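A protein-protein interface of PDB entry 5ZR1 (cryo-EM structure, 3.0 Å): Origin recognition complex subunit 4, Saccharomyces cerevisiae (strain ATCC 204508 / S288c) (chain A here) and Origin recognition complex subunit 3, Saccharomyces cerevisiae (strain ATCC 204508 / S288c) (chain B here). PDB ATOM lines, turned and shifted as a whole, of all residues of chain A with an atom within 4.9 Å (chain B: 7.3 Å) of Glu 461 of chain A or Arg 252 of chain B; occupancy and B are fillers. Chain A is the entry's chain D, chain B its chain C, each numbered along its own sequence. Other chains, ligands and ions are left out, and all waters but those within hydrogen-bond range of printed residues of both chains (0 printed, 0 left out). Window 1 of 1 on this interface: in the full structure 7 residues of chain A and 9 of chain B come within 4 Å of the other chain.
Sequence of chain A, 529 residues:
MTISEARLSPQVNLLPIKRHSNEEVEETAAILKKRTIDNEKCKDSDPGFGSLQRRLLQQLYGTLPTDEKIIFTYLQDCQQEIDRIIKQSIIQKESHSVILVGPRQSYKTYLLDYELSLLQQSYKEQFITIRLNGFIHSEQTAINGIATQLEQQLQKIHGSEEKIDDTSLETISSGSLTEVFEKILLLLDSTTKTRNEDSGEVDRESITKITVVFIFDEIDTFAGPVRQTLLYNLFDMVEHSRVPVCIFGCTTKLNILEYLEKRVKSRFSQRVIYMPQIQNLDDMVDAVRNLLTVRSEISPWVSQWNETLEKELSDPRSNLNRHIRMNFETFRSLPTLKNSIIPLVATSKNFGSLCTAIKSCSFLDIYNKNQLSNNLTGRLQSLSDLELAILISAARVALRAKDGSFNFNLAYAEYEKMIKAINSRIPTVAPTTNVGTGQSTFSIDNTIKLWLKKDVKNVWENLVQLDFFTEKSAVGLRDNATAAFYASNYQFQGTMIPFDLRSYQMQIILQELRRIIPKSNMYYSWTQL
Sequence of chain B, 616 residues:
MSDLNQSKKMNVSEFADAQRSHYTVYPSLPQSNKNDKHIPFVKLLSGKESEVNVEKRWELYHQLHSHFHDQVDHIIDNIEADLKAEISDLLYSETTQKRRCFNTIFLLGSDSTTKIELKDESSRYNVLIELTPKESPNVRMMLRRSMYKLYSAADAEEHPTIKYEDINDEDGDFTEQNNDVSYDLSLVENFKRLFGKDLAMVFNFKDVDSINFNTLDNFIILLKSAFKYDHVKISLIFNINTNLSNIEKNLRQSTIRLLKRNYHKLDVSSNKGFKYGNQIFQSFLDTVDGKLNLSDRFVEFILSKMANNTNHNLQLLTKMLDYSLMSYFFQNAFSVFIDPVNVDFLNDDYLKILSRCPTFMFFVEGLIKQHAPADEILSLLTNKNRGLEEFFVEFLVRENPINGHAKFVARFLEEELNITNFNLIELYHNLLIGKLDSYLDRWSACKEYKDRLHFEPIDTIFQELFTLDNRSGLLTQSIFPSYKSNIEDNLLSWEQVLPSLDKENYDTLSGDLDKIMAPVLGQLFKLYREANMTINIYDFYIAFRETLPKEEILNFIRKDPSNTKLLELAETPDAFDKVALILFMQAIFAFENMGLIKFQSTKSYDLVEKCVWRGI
O of Leu 251 of chain B is in hydrogen-bond range of NZ of Lys 457 of chain A (3.1 Å).
The backbone NH (N) of Gln 253 of chain B lies within hydrogen-bond range of the side-chain carboxylate (OE1) of Glu 461 of chain A.
The guanidinium group (NH1) of Arg 257 of chain B lies close to the side-chain amide nitrogen (ND2) of Asn 458 of chain A, 3.1 Å away.
The guanidinium group (NE) of Arg 252 of chain B is in salt-bridge range of the side-chain carboxylate (OD2) of Asp 217 of chain B, 3.3 Å away.
The side-chain amide oxygen (OD1) of Asn 218 of chain B sits at hydrogen-bond distance from the guanidinium group (NH2) of Arg 252 of chain B (3.2 Å).
OE2 of Glu 248 of chain B is in salt-bridge range of NZ of Lys 249 of chain B, at 3.7 Å.
The side-chain amino group of Lys 457 of chain A lies within salt-bridge range of the side-chain carboxylate of Glu 461 of chain A.
The backbone carbonyl oxygen (O) of Asn 458 of chain A is in hydrogen-bond range of the side-chain amide nitrogen (ND2) of Asn 462 of chain A (3.0 Å).
Among the printed residues, merely in contact across the chains: Phe 499 of chain A with Lys 249 of chain B (3.4 Å), Glu 461 of chain A with Arg 252 of chain B (3.6 Å), Lys 457 of chain A with Gln 253 of chain B (3.8 Å) and Asn 458 of chain A with Gln 253 of chain B (3.9 Å).
Of the printed residues of chain B, Glu 461 of chain A touches Arg 252 and Gln 253.
Of chain A, only Glu 461 comes within 4 Å of Arg 252 of chain B.
Printed residues of chain A within 4 Å of Leu 251 of chain B: Lys 457 (3.1 Å).
Of the printed residues of chain A, Gln 253 of chain B touches Lys 457 (3.8 Å), Asn 458 (3.9 Å) and Glu 461 (2.9 Å).
Printed residues of chain A within 4 Å of Arg 257 of chain B: Asn 458 (3.1 Å).
Of the printed residues of chain B, Lys 457 of chain A touches Leu 251 (3.1 Å) and Gln 253 (3.8 Å).
Trp 460 of chain A touches none of the printed residues of chain B.
The nearest residue of chain B that does not touch Glu 461 of chain A is Leu 251 of chain B (4.2 Å).
The nearest residue of chain A that does not touch Arg 252 of chain B is Lys 457 of chain A (4.04 Å).
The nearest printed residue of chain A that does not touch Leu 251 of chain B is Glu 461 of chain A (4.2 Å).
Hydrophobic or aromatic side chains of chain A that line the printed part of chain B: Phe 499.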
ATOM      1  N   LYS A 457      19.114 -26.349  21.198  1.00  0.00           N
ATOM      2  CA  LYS A 457      17.692 -26.632  21.403  1.00  0.00           C
ATOM      3  C   LYS A 457      16.850 -25.358  21.423  1.00  0.00           C
ATOM      4  O   LYS A 457      15.734 -25.340  20.894  1.00  0.00           O
ATOM      5  CB  LYS A 457      17.502 -27.407  22.707  1.00  0.00           C
ATOM      6  CG  LYS A 457      16.068 -27.791  22.994  1.00  0.00           C
ATOM      7  CD  LYS A 457      15.920 -28.531  24.301  1.00  0.00           C
ATOM      8  CE  LYS A 457      14.489 -28.990  24.486  1.00  0.00           C
ATOM      9  NZ  LYS A 457      13.560 -27.844  24.637  1.00  0.00           N
ATOM     10  N   ASN A 458      17.382 -24.276  21.993  1.00  0.00           N
ATOM     11  CA  ASN A 458      16.672 -23.001  21.961  1.00  0.00           C
ATOM     12  C   ASN A 458      16.653 -22.418  20.552  1.00  0.00           C
ATOM     13  O   ASN A 458      15.649 -21.837  20.127  1.00  0.00           O
ATOM     14  CB  ASN A 458      17.322 -22.019  22.931  1.00  0.00           C
ATOM     15  CG  ASN A 458      16.457 -20.812  23.216  1.00  0.00           C
ATOM     16  OD1 ASN A 458      15.309 -20.737  22.790  1.00  0.00           O
ATOM     17  ND2 ASN A 458      17.017 -19.845  23.921  1.00  0.00           N
ATOM     18  N   VAL A 459      17.761 -22.556  19.822  1.00  0.00           N
ATOM     19  CA  VAL A 459      17.832 -22.109  18.434  1.00  0.00           C
ATOM     20  C   VAL A 459      16.913 -22.942  17.553  1.00  0.00           C
ATOM     21  O   VAL A 459      16.280 -22.413  16.630  1.00  0.00           O
ATOM     22  CB  VAL A 459      19.303 -22.155  17.974  1.00  0.00           C
ATOM     23  CG1 VAL A 459      19.445 -21.966  16.484  1.00  0.00           C
ATOM     24  CG2 VAL A 459      20.086 -21.083  18.687  1.00  0.00           C
ATOM     25  N   TRP A 460      16.778 -24.234  17.858  1.00  0.00           N
ATOM     26  CA  TRP A 460      15.918 -25.114  17.074  1.00  0.00           C
ATOM     27  C   TRP A 460      14.452 -24.734  17.219  1.00  0.00           C
ATOM     28  O   TRP A 460      13.693 -24.795  16.248  1.00  0.00           O
ATOM     29  CB  TRP A 460      16.122 -26.555  17.511  1.00  0.00           C
ATOM     30  CG  TRP A 460      15.449 -27.529  16.637  1.00  0.00           C
ATOM     31  CD1 TRP A 460      14.279 -28.176  16.869  1.00  0.00           C
ATOM     32  CD2 TRP A 460      15.916 -27.982  15.373  1.00  0.00           C
ATOM     33  NE1 TRP A 460      13.985 -29.012  15.822  1.00  0.00           N
ATOM     34  CE2 TRP A 460      14.984 -28.912  14.890  1.00  0.00           C
ATOM     35  CE3 TRP A 460      17.045 -27.698  14.607  1.00  0.00           C
ATOM     36  CZ2 TRP A 460      15.140 -29.550  13.673  1.00  0.00           C
ATOM     37  CZ3 TRP A 460      17.198 -28.326  13.408  1.00  0.00           C
ATOM     38  CH2 TRP A 460      16.256 -29.246  12.948  1.00  0.00           C
ATOM     39  N   GLU A 461      14.042 -24.325  18.414  1.00  0.00           N
ATOM     40  CA  GLU A 461      12.650 -23.990  18.663  1.00  0.00           C
ATOM     41  C   GLU A 461      12.274 -22.611  18.154  1.00  0.00           C
ATOM     42  O   GLU A 461      11.085 -22.348  17.954  1.00  0.00           O
ATOM     43  CB  GLU A 461      12.366 -24.086  20.158  1.00  0.00           C
ATOM     44  CG  GLU A 461      12.468 -25.497  20.687  1.00  0.00           C
ATOM     45  CD  GLU A 461      12.417 -25.554  22.193  1.00  0.00           C
ATOM     46  OE1 GLU A 461      12.424 -24.479  22.828  1.00  0.00           O
ATOM     47  OE2 GLU A 461      12.388 -26.674  22.742  1.00  0.00           O
ATOM     48  N   ASN A 462      13.246 -21.726  17.943  1.00  0.00           N
ATOM     49  CA  ASN A 462      12.925 -20.422  17.380  1.00  0.00           C
ATOM     50  C   ASN A 462      12.727 -20.499  15.877  1.00  0.00           C
ATOM     51  O   ASN A 462      11.898 -19.771  15.328  1.00  0.00           O
ATOM     52  CB  ASN A 462      14.021 -19.415  17.712  1.00  0.00           C
ATOM     53  CG  ASN A 462      14.127 -19.151  19.192  1.00  0.00           C
ATOM     54  OD1 ASN A 462      13.125 -19.130  19.902  1.00  0.00           O
ATOM     55  ND2 ASN A 462      15.342 -18.924  19.665  1.00  0.00           N
ATOM     56  N   LEU A 463      13.464 -21.378  15.203  1.00  0.00           N
ATOM     57  CA  LEU A 463      13.252 -21.596  13.781  1.00  0.00           C
ATOM     58  C   LEU A 463      11.946 -22.321  13.507  1.00  0.00           C
ATOM     59  O   LEU A 463      11.422 -22.234  12.395  1.00  0.00           O
ATOM     60  CB  LEU A 463      14.418 -22.390  13.205  1.00  0.00           C
ATOM     61  CG  LEU A 463      15.780 -21.713  13.309  1.00  0.00           C
ATOM     62  CD1 LEU A 463      16.855 -22.667  12.867  1.00  0.00           C
ATOM     63  CD2 LEU A 463      15.817 -20.448  12.481  1.00  0.00           C
ATOM     64  N   VAL A 464      11.427 -23.054  14.491  1.00  0.00           N
ATOM     65  CA  VAL A 464      10.090 -23.623  14.378  1.00  0.00           C
ATOM     66  C   VAL A 464       9.039 -22.523  14.443  1.00  0.00           C
ATOM     67  O   VAL A 464       8.125 -22.468  13.613  1.00  0.00           O
ATOM     68  CB  VAL A 464       9.871 -24.685  15.471  1.00  0.00           C
ATOM     69  CG1 VAL A 464       8.430 -25.138  15.497  1.00  0.00           C
ATOM     70  CG2 VAL A 464      10.761 -25.872  15.220  1.00  0.00           C
ATOM     71  N   GLN A 465       9.164 -21.611  15.408  1.00  0.00           N
ATOM     72  CA  GLN A 465       8.115 -20.618  15.596  1.00  0.00           C
ATOM     73  C   GLN A 465       8.234 -19.423  14.663  1.00  0.00           C
ATOM     74  O   GLN A 465       7.340 -18.573  14.666  1.00  0.00           O
ATOM     75  CB  GLN A 465       8.083 -20.121  17.040  1.00  0.00           C
ATOM     76  CG  GLN A 465       9.242 -19.252  17.439  1.00  0.00           C
ATOM     77  CD  GLN A 465       9.077 -18.719  18.846  1.00  0.00           C
ATOM     78  OE1 GLN A 465       8.067 -18.971  19.498  1.00  0.00           O
ATOM     79  NE2 GLN A 465      10.065 -17.968  19.316  1.00  0.00           N
ATOM     80  N   PHE A 499      11.793 -35.054  21.718  1.00  0.00           N
ATOM     81  CA  PHE A 499      12.049 -33.784  21.044  1.00  0.00           C
ATOM     82  C   PHE A 499      12.934 -33.956  19.817  1.00  0.00           C
ATOM     83  O   PHE A 499      12.582 -33.518  18.717  1.00  0.00           O
ATOM     84  CB  PHE A 499      12.692 -32.803  22.024  1.00  0.00           C
ATOM     85  CG  PHE A 499      13.151 -31.530  21.386  1.00  0.00           C
ATOM     86  CD1 PHE A 499      12.238 -30.562  21.015  1.00  0.00           C
ATOM     87  CD2 PHE A 499      14.502 -31.302  21.154  1.00  0.00           C
ATOM     88  CE1 PHE A 499      12.656 -29.390  20.420  1.00  0.00           C
ATOM     89  CE2 PHE A 499      14.926 -30.143  20.554  1.00  0.00           C
ATOM     90  CZ  PHE A 499      14.004 -29.179  20.192  1.00  0.00           C
ATOM     91  N   PHE B 213       3.021 -33.104  26.786  1.00  0.00           N
ATOM     92  CA  PHE B 213       3.706 -31.891  27.186  1.00  0.00           C
ATOM     93  C   PHE B 213       3.509 -30.750  26.208  1.00  0.00           C
ATOM     94  O   PHE B 213       4.020 -29.661  26.453  1.00  0.00           O
ATOM     95  CB  PHE B 213       5.191 -32.179  27.372  1.00  0.00           C
ATOM     96  CG  PHE B 213       5.481 -33.092  28.517  1.00  0.00           C
ATOM     97  CD1 PHE B 213       5.607 -32.593  29.800  1.00  0.00           C
ATOM     98  CD2 PHE B 213       5.594 -34.457  28.317  1.00  0.00           C
ATOM     99  CE1 PHE B 213       5.868 -33.436  30.853  1.00  0.00           C
ATOM    100  CE2 PHE B 213       5.849 -35.301  29.368  1.00  0.00           C
ATOM    101  CZ  PHE B 213       5.986 -34.790  30.631  1.00  0.00           C
ATOM    102  N   ASN B 214       2.802 -30.974  25.100  1.00  0.00           N
ATOM    103  CA  ASN B 214       2.364 -29.853  24.278  1.00  0.00           C
ATOM    104  C   ASN B 214       1.257 -29.086  24.978  1.00  0.00           C
ATOM    105  O   ASN B 214       1.205 -27.854  24.918  1.00  0.00           O
ATOM    106  CB  ASN B 214       1.869 -30.353  22.924  1.00  0.00           C
ATOM    107  CG  ASN B 214       1.947 -29.302  21.836  1.00  0.00           C
ATOM    108  OD1 ASN B 214       1.698 -29.594  20.668  1.00  0.00           O
ATOM    109  ND2 ASN B 214       2.342 -28.089  22.197  1.00  0.00           N
ATOM    110  N   THR B 215       0.358 -29.809  25.639  1.00  0.00           N
ATOM    111  CA  THR B 215      -0.783 -29.198  26.297  1.00  0.00           C
ATOM    112  C   THR B 215      -0.369 -28.513  27.591  1.00  0.00           C
ATOM    113  O   THR B 215      -0.823 -27.403  27.885  1.00  0.00           O
ATOM    114  CB  THR B 215      -1.844 -30.266  26.557  1.00  0.00           C
ATOM    115  OG1 THR B 215      -2.169 -30.917  25.325  1.00  0.00           O
ATOM    116  CG2 THR B 215      -3.090 -29.649  27.093  1.00  0.00           C
ATOM    117  N   ASP B 217       2.621 -27.379  28.311  1.00  0.00           N
ATOM    118  CA  ASP B 217       3.414 -26.199  27.984  1.00  0.00           C
ATOM    119  C   ASP B 217       2.515 -25.029  27.616  1.00  0.00           C
ATOM    120  O   ASP B 217       2.741 -23.904  28.066  1.00  0.00           O
ATOM    121  CB  ASP B 217       4.367 -26.521  26.838  1.00  0.00           C
ATOM    122  CG  ASP B 217       5.468 -25.504  26.674  1.00  0.00           C
ATOM    123  OD1 ASP B 217       5.518 -24.512  27.426  1.00  0.00           O
ATOM    124  OD2 ASP B 217       6.305 -25.710  25.779  1.00  0.00           O
ATOM    125  N   ASN B 218       1.476 -25.283  26.820  1.00  0.00           N
ATOM    126  CA  ASN B 218       0.576 -24.217  26.401  1.00  0.00           C
ATOM    127  C   ASN B 218      -0.331 -23.742  27.523  1.00  0.00           C
ATOM    128  O   ASN B 218      -0.919 -22.664  27.409  1.00  0.00           O
ATOM    129  CB  ASN B 218      -0.284 -24.675  25.229  1.00  0.00           C
ATOM    130  CG  ASN B 218       0.516 -24.898  23.974  1.00  0.00           C
ATOM    131  OD1 ASN B 218       1.437 -24.147  23.670  1.00  0.00           O
ATOM    132  ND2 ASN B 218       0.156 -25.926  23.221  1.00  0.00           N
ATOM    133  N   PHE B 219      -0.470 -24.516  28.594  1.00  0.00           N
ATOM    134  CA  PHE B 219      -1.295 -24.092  29.713  1.00  0.00           C
ATOM    135  C   PHE B 219      -0.508 -23.281  30.731  1.00  0.00           C
ATOM    136  O   PHE B 219      -1.076 -22.390  31.367  1.00  0.00           O
ATOM    137  CB  PHE B 219      -1.933 -25.308  30.382  1.00  0.00           C
ATOM    138  CG  PHE B 219      -2.918 -24.965  31.454  1.00  0.00           C
ATOM    139  CD1 PHE B 219      -4.146 -24.424  31.128  1.00  0.00           C
ATOM    140  CD2 PHE B 219      -2.628 -25.206  32.784  1.00  0.00           C
ATOM    141  CE1 PHE B 219      -5.058 -24.113  32.108  1.00  0.00           C
ATOM    142  CE2 PHE B 219      -3.537 -24.897  33.768  1.00  0.00           C
ATOM    143  CZ  PHE B 219      -4.753 -24.353  33.428  1.00  0.00           C
ATOM    144  N   ILE B 221       1.991 -21.317  29.771  1.00  0.00           N
ATOM    145  CA  ILE B 221       2.047 -20.061  29.026  1.00  0.00           C
ATOM    146  C   ILE B 221       0.711 -19.325  29.106  1.00  0.00           C
ATOM    147  O   ILE B 221       0.674 -18.089  29.154  1.00  0.00           O
ATOM    148  CB  ILE B 221       2.478 -20.363  27.575  1.00  0.00           C
ATOM    149  CG1 ILE B 221       3.905 -20.899  27.558  1.00  0.00           C
ATOM    150  CG2 ILE B 221       2.408 -19.144  26.680  1.00  0.00           C
ATOM    151  CD1 ILE B 221       4.322 -21.444  26.223  1.00  0.00           C
ATOM    152  N   ILE B 247      11.573 -34.329  31.952  1.00  0.00           N
ATOM    153  CA  ILE B 247      10.565 -33.291  31.782  1.00  0.00           C
ATOM    154  C   ILE B 247      11.141 -32.096  31.039  1.00  0.00           C
ATOM    155  O   ILE B 247      10.477 -31.504  30.182  1.00  0.00           O
ATOM    156  CB  ILE B 247       9.995 -32.890  33.152  1.00  0.00           C
ATOM    157  CG1 ILE B 247       9.523 -34.133  33.896  1.00  0.00           C
ATOM    158  CG2 ILE B 247       8.840 -31.922  33.005  1.00  0.00           C
ATOM    159  CD1 ILE B 247       8.454 -34.919  33.198  1.00  0.00           C
ATOM    160  N   GLU B 248      12.387 -31.734  31.334  1.00  0.00           N
ATOM    161  CA  GLU B 248      13.001 -30.582  30.691  1.00  0.00           C
ATOM    162  C   GLU B 248      13.448 -30.858  29.261  1.00  0.00           C
ATOM    163  O   GLU B 248      13.805 -29.914  28.552  1.00  0.00           O
ATOM    164  CB  GLU B 248      14.179 -30.080  31.529  1.00  0.00           C
ATOM    165  CG  GLU B 248      15.319 -31.065  31.679  1.00  0.00           C
ATOM    166  CD  GLU B 248      16.394 -30.557  32.620  1.00  0.00           C
ATOM    167  OE1 GLU B 248      16.227 -29.447  33.171  1.00  0.00           O
ATOM    168  OE2 GLU B 248      17.405 -31.263  32.811  1.00  0.00           O
ATOM    169  N   LYS B 249      13.443 -32.113  28.815  1.00  0.00           N
ATOM    170  CA  LYS B 249      13.612 -32.389  27.396  1.00  0.00           C
ATOM    171  C   LYS B 249      12.296 -32.320  26.636  1.00  0.00           C
ATOM    172  O   LYS B 249      12.310 -32.302  25.403  1.00  0.00           O
ATOM    173  CB  LYS B 249      14.239 -33.765  27.185  1.00  0.00           C
ATOM    174  CG  LYS B 249      15.548 -33.966  27.910  1.00  0.00           C
ATOM    175  CD  LYS B 249      16.626 -33.021  27.437  1.00  0.00           C
ATOM    176  CE  LYS B 249      17.934 -33.314  28.150  1.00  0.00           C
ATOM    177  NZ  LYS B 249      17.863 -32.955  29.594  1.00  0.00           N
ATOM    178  N   ASN B 250      11.170 -32.278  27.344  1.00  0.00           N
ATOM    179  CA  ASN B 250       9.846 -32.273  26.733  1.00  0.00           C
ATOM    180  C   ASN B 250       9.275 -30.870  26.603  1.00  0.00           C
ATOM    181  O   ASN B 250       8.684 -30.535  25.571  1.00  0.00           O
ATOM    182  CB  ASN B 250       8.895 -33.138  27.557  1.00  0.00           C
ATOM    183  CG  ASN B 250       9.237 -34.607  27.489  1.00  0.00           C
ATOM    184  OD1 ASN B 250       9.518 -35.142  26.419  1.00  0.00           O
ATOM    185  ND2 ASN B 250       9.228 -35.266  28.638  1.00  0.00           N
ATOM    186  N   LEU B 251       9.427 -30.049  27.636  1.00  0.00           N
ATOM    187  CA  LEU B 251       8.958 -28.675  27.586  1.00  0.00           C
ATOM    188  C   LEU B 251       9.859 -27.843  26.686  1.00  0.00           C
ATOM    189  O   LEU B 251      11.031 -28.164  26.477  1.00  0.00           O
ATOM    190  CB  LEU B 251       8.933 -28.074  28.988  1.00  0.00           C
ATOM    191  CG  LEU B 251       7.982 -28.714  29.993  1.00  0.00           C
ATOM    192  CD1 LEU B 251       8.239 -28.133  31.353  1.00  0.00           C
ATOM    193  CD2 LEU B 251       6.543 -28.485  29.594  1.00  0.00           C
ATOM    194  N   ARG B 252       9.301 -26.767  26.141  1.00  0.00           N
ATOM    195  CA  ARG B 252      10.110 -25.857  25.351  1.00  0.00           C
ATOM    196  C   ARG B 252      11.027 -25.052  26.263  1.00  0.00           C
ATOM    197  O   ARG B 252      10.786 -24.914  27.465  1.00  0.00           O
ATOM    198  CB  ARG B 252       9.232 -24.932  24.508  1.00  0.00           C
ATOM    199  CG  ARG B 252       8.530 -25.636  23.356  1.00  0.00           C
ATOM    200  CD  ARG B 252       7.862 -24.650  22.414  1.00  0.00           C
ATOM    201  NE  ARG B 252       6.762 -23.925  23.039  1.00  0.00           N
ATOM    202  CZ  ARG B 252       5.499 -24.342  23.042  1.00  0.00           C
ATOM    203  NH1 ARG B 252       5.174 -25.483  22.455  1.00  0.00           N
ATOM    204  NH2 ARG B 252       4.561 -23.619  23.633  1.00  0.00           N
ATOM    205  N   GLN B 253      12.097 -24.521  25.669  1.00  0.00           N
ATOM    206  CA  GLN B 253      13.184 -23.931  26.444  1.00  0.00           C
ATOM    207  C   GLN B 253      12.770 -22.629  27.117  1.00  0.00           C
ATOM    208  O   GLN B 253      13.242 -22.326  28.217  1.00  0.00           O
ATOM    209  CB  GLN B 253      14.394 -23.718  25.535  1.00  0.00           C
ATOM    210  CG  GLN B 253      15.654 -23.255  26.236  1.00  0.00           C
ATOM    211  CD  GLN B 253      16.142 -24.247  27.262  1.00  0.00           C
ATOM    212  OE1 GLN B 253      16.008 -24.028  28.464  1.00  0.00           O
ATOM    213  NE2 GLN B 253      16.705 -25.353  26.794  1.00  0.00           N
ATOM    214  N   SER B 254      11.868 -21.867  26.501  1.00  0.00           N
ATOM    215  CA  SER B 254      11.404 -20.621  27.094  1.00  0.00           C
ATOM    216  C   SER B 254      10.438 -20.832  28.252  1.00  0.00           C
ATOM    217  O   SER B 254      10.156 -19.875  28.978  1.00  0.00           O
ATOM    218  CB  SER B 254      10.740 -19.753  26.028  1.00  0.00           C
ATOM    219  OG  SER B 254       9.564 -20.367  25.537  1.00  0.00           O
ATOM    220  N   THR B 255       9.920 -22.045  28.434  1.00  0.00           N
ATOM    221  CA  THR B 255       9.059 -22.368  29.562  1.00  0.00           C
ATOM    222  C   THR B 255       9.878 -22.735  30.791  1.00  0.00           C
ATOM    223  O   THR B 255       9.512 -22.382  31.918  1.00  0.00           O
ATOM    224  CB  THR B 255       8.125 -23.519  29.180  1.00  0.00           C
ATOM    225  OG1 THR B 255       7.419 -23.171  27.985  1.00  0.00           O
ATOM    226  CG2 THR B 255       7.104 -23.792  30.272  1.00  0.00           C
ATOM    227  N   ILE B 256      10.995 -23.427  30.576  1.00  0.00           N
ATOM    228  CA  ILE B 256      11.913 -23.788  31.649  1.00  0.00           C
ATOM    229  C   ILE B 256      12.548 -22.547  32.258  1.00  0.00           C
ATOM    230  O   ILE B 256      12.761 -22.480  33.473  1.00  0.00           O
ATOM    231  CB  ILE B 256      12.953 -24.768  31.083  1.00  0.00           C
ATOM    232  CG1 ILE B 256      12.251 -26.032  30.601  1.00  0.00           C
ATOM    233  CG2 ILE B 256      14.015 -25.115  32.093  1.00  0.00           C
ATOM    234  CD1 ILE B 256      13.134 -26.918  29.787  1.00  0.00           C
ATOM    235  N   ARG B 257      12.814 -21.528  31.440  1.00  0.00           N
ATOM    236  CA  ARG B 257      13.283 -20.253  31.965  1.00  0.00           C
ATOM    237  C   ARG B 257      12.216 -19.533  32.778  1.00  0.00           C
ATOM    238  O   ARG B 257      12.558 -18.691  33.611  1.00  0.00           O
ATOM    239  CB  ARG B 257      13.766 -19.355  30.827  1.00  0.00           C
ATOM    240  CG  ARG B 257      15.028 -19.851  30.158  1.00  0.00           C
ATOM    241  CD  ARG B 257      15.680 -18.761  29.332  1.00  0.00           C
ATOM    242  NE  ARG B 257      14.872 -18.344  28.194  1.00  0.00           N
ATOM    243  CZ  ARG B 257      14.958 -18.885  26.988  1.00  0.00           C
ATOM    244  NH1 ARG B 257      15.816 -19.868  26.765  1.00  0.00           N
ATOM    245  NH2 ARG B 257      14.186 -18.446  26.006  1.00  0.00           N
ATOM    246  N   LEU B 258      10.939 -19.841  32.553  1.00  0.00           N
ATOM    247  CA  LEU B 258       9.873 -19.317  33.396  1.00  0.00           C
ATOM    248  C   LEU B 258       9.736 -20.112  34.688  1.00  0.00           C
ATOM    249  O   LEU B 258       9.431 -19.535  35.736  1.00  0.00           O
ATOM    250  CB  LEU B 258       8.553 -19.331  32.625  1.00  0.00           C
ATOM    251  CG  LEU B 258       7.299 -18.782  33.300  1.00  0.00           C
ATOM    252  CD1 LEU B 258       7.407 -17.286  33.521  1.00  0.00           C
ATOM    253  CD2 LEU B 258       6.072 -19.136  32.487  1.00  0.00           C
ATOM    254  N   LEU B 259       9.975 -21.423  34.635  1.00  0.00           N
ATOM    255  CA  LEU B 259       9.864 -22.312  35.787  1.00  0.00           C
ATOM    256  C   LEU B 259      11.045 -22.223  36.744  1.00  0.00           C
ATOM    257  O   LEU B 259      11.052 -22.942  37.745  1.00  0.00           O
ATOM    258  CB  LEU B 259       9.737 -23.768  35.326  1.00  0.00           C
ATOM    259  CG  LEU B 259       8.530 -24.271  34.539  1.00  0.00           C
ATOM    260  CD1 LEU B 259       8.811 -25.664  34.045  1.00  0.00           C
ATOM    261  CD2 LEU B 259       7.318 -24.312  35.398  1.00  0.00           C
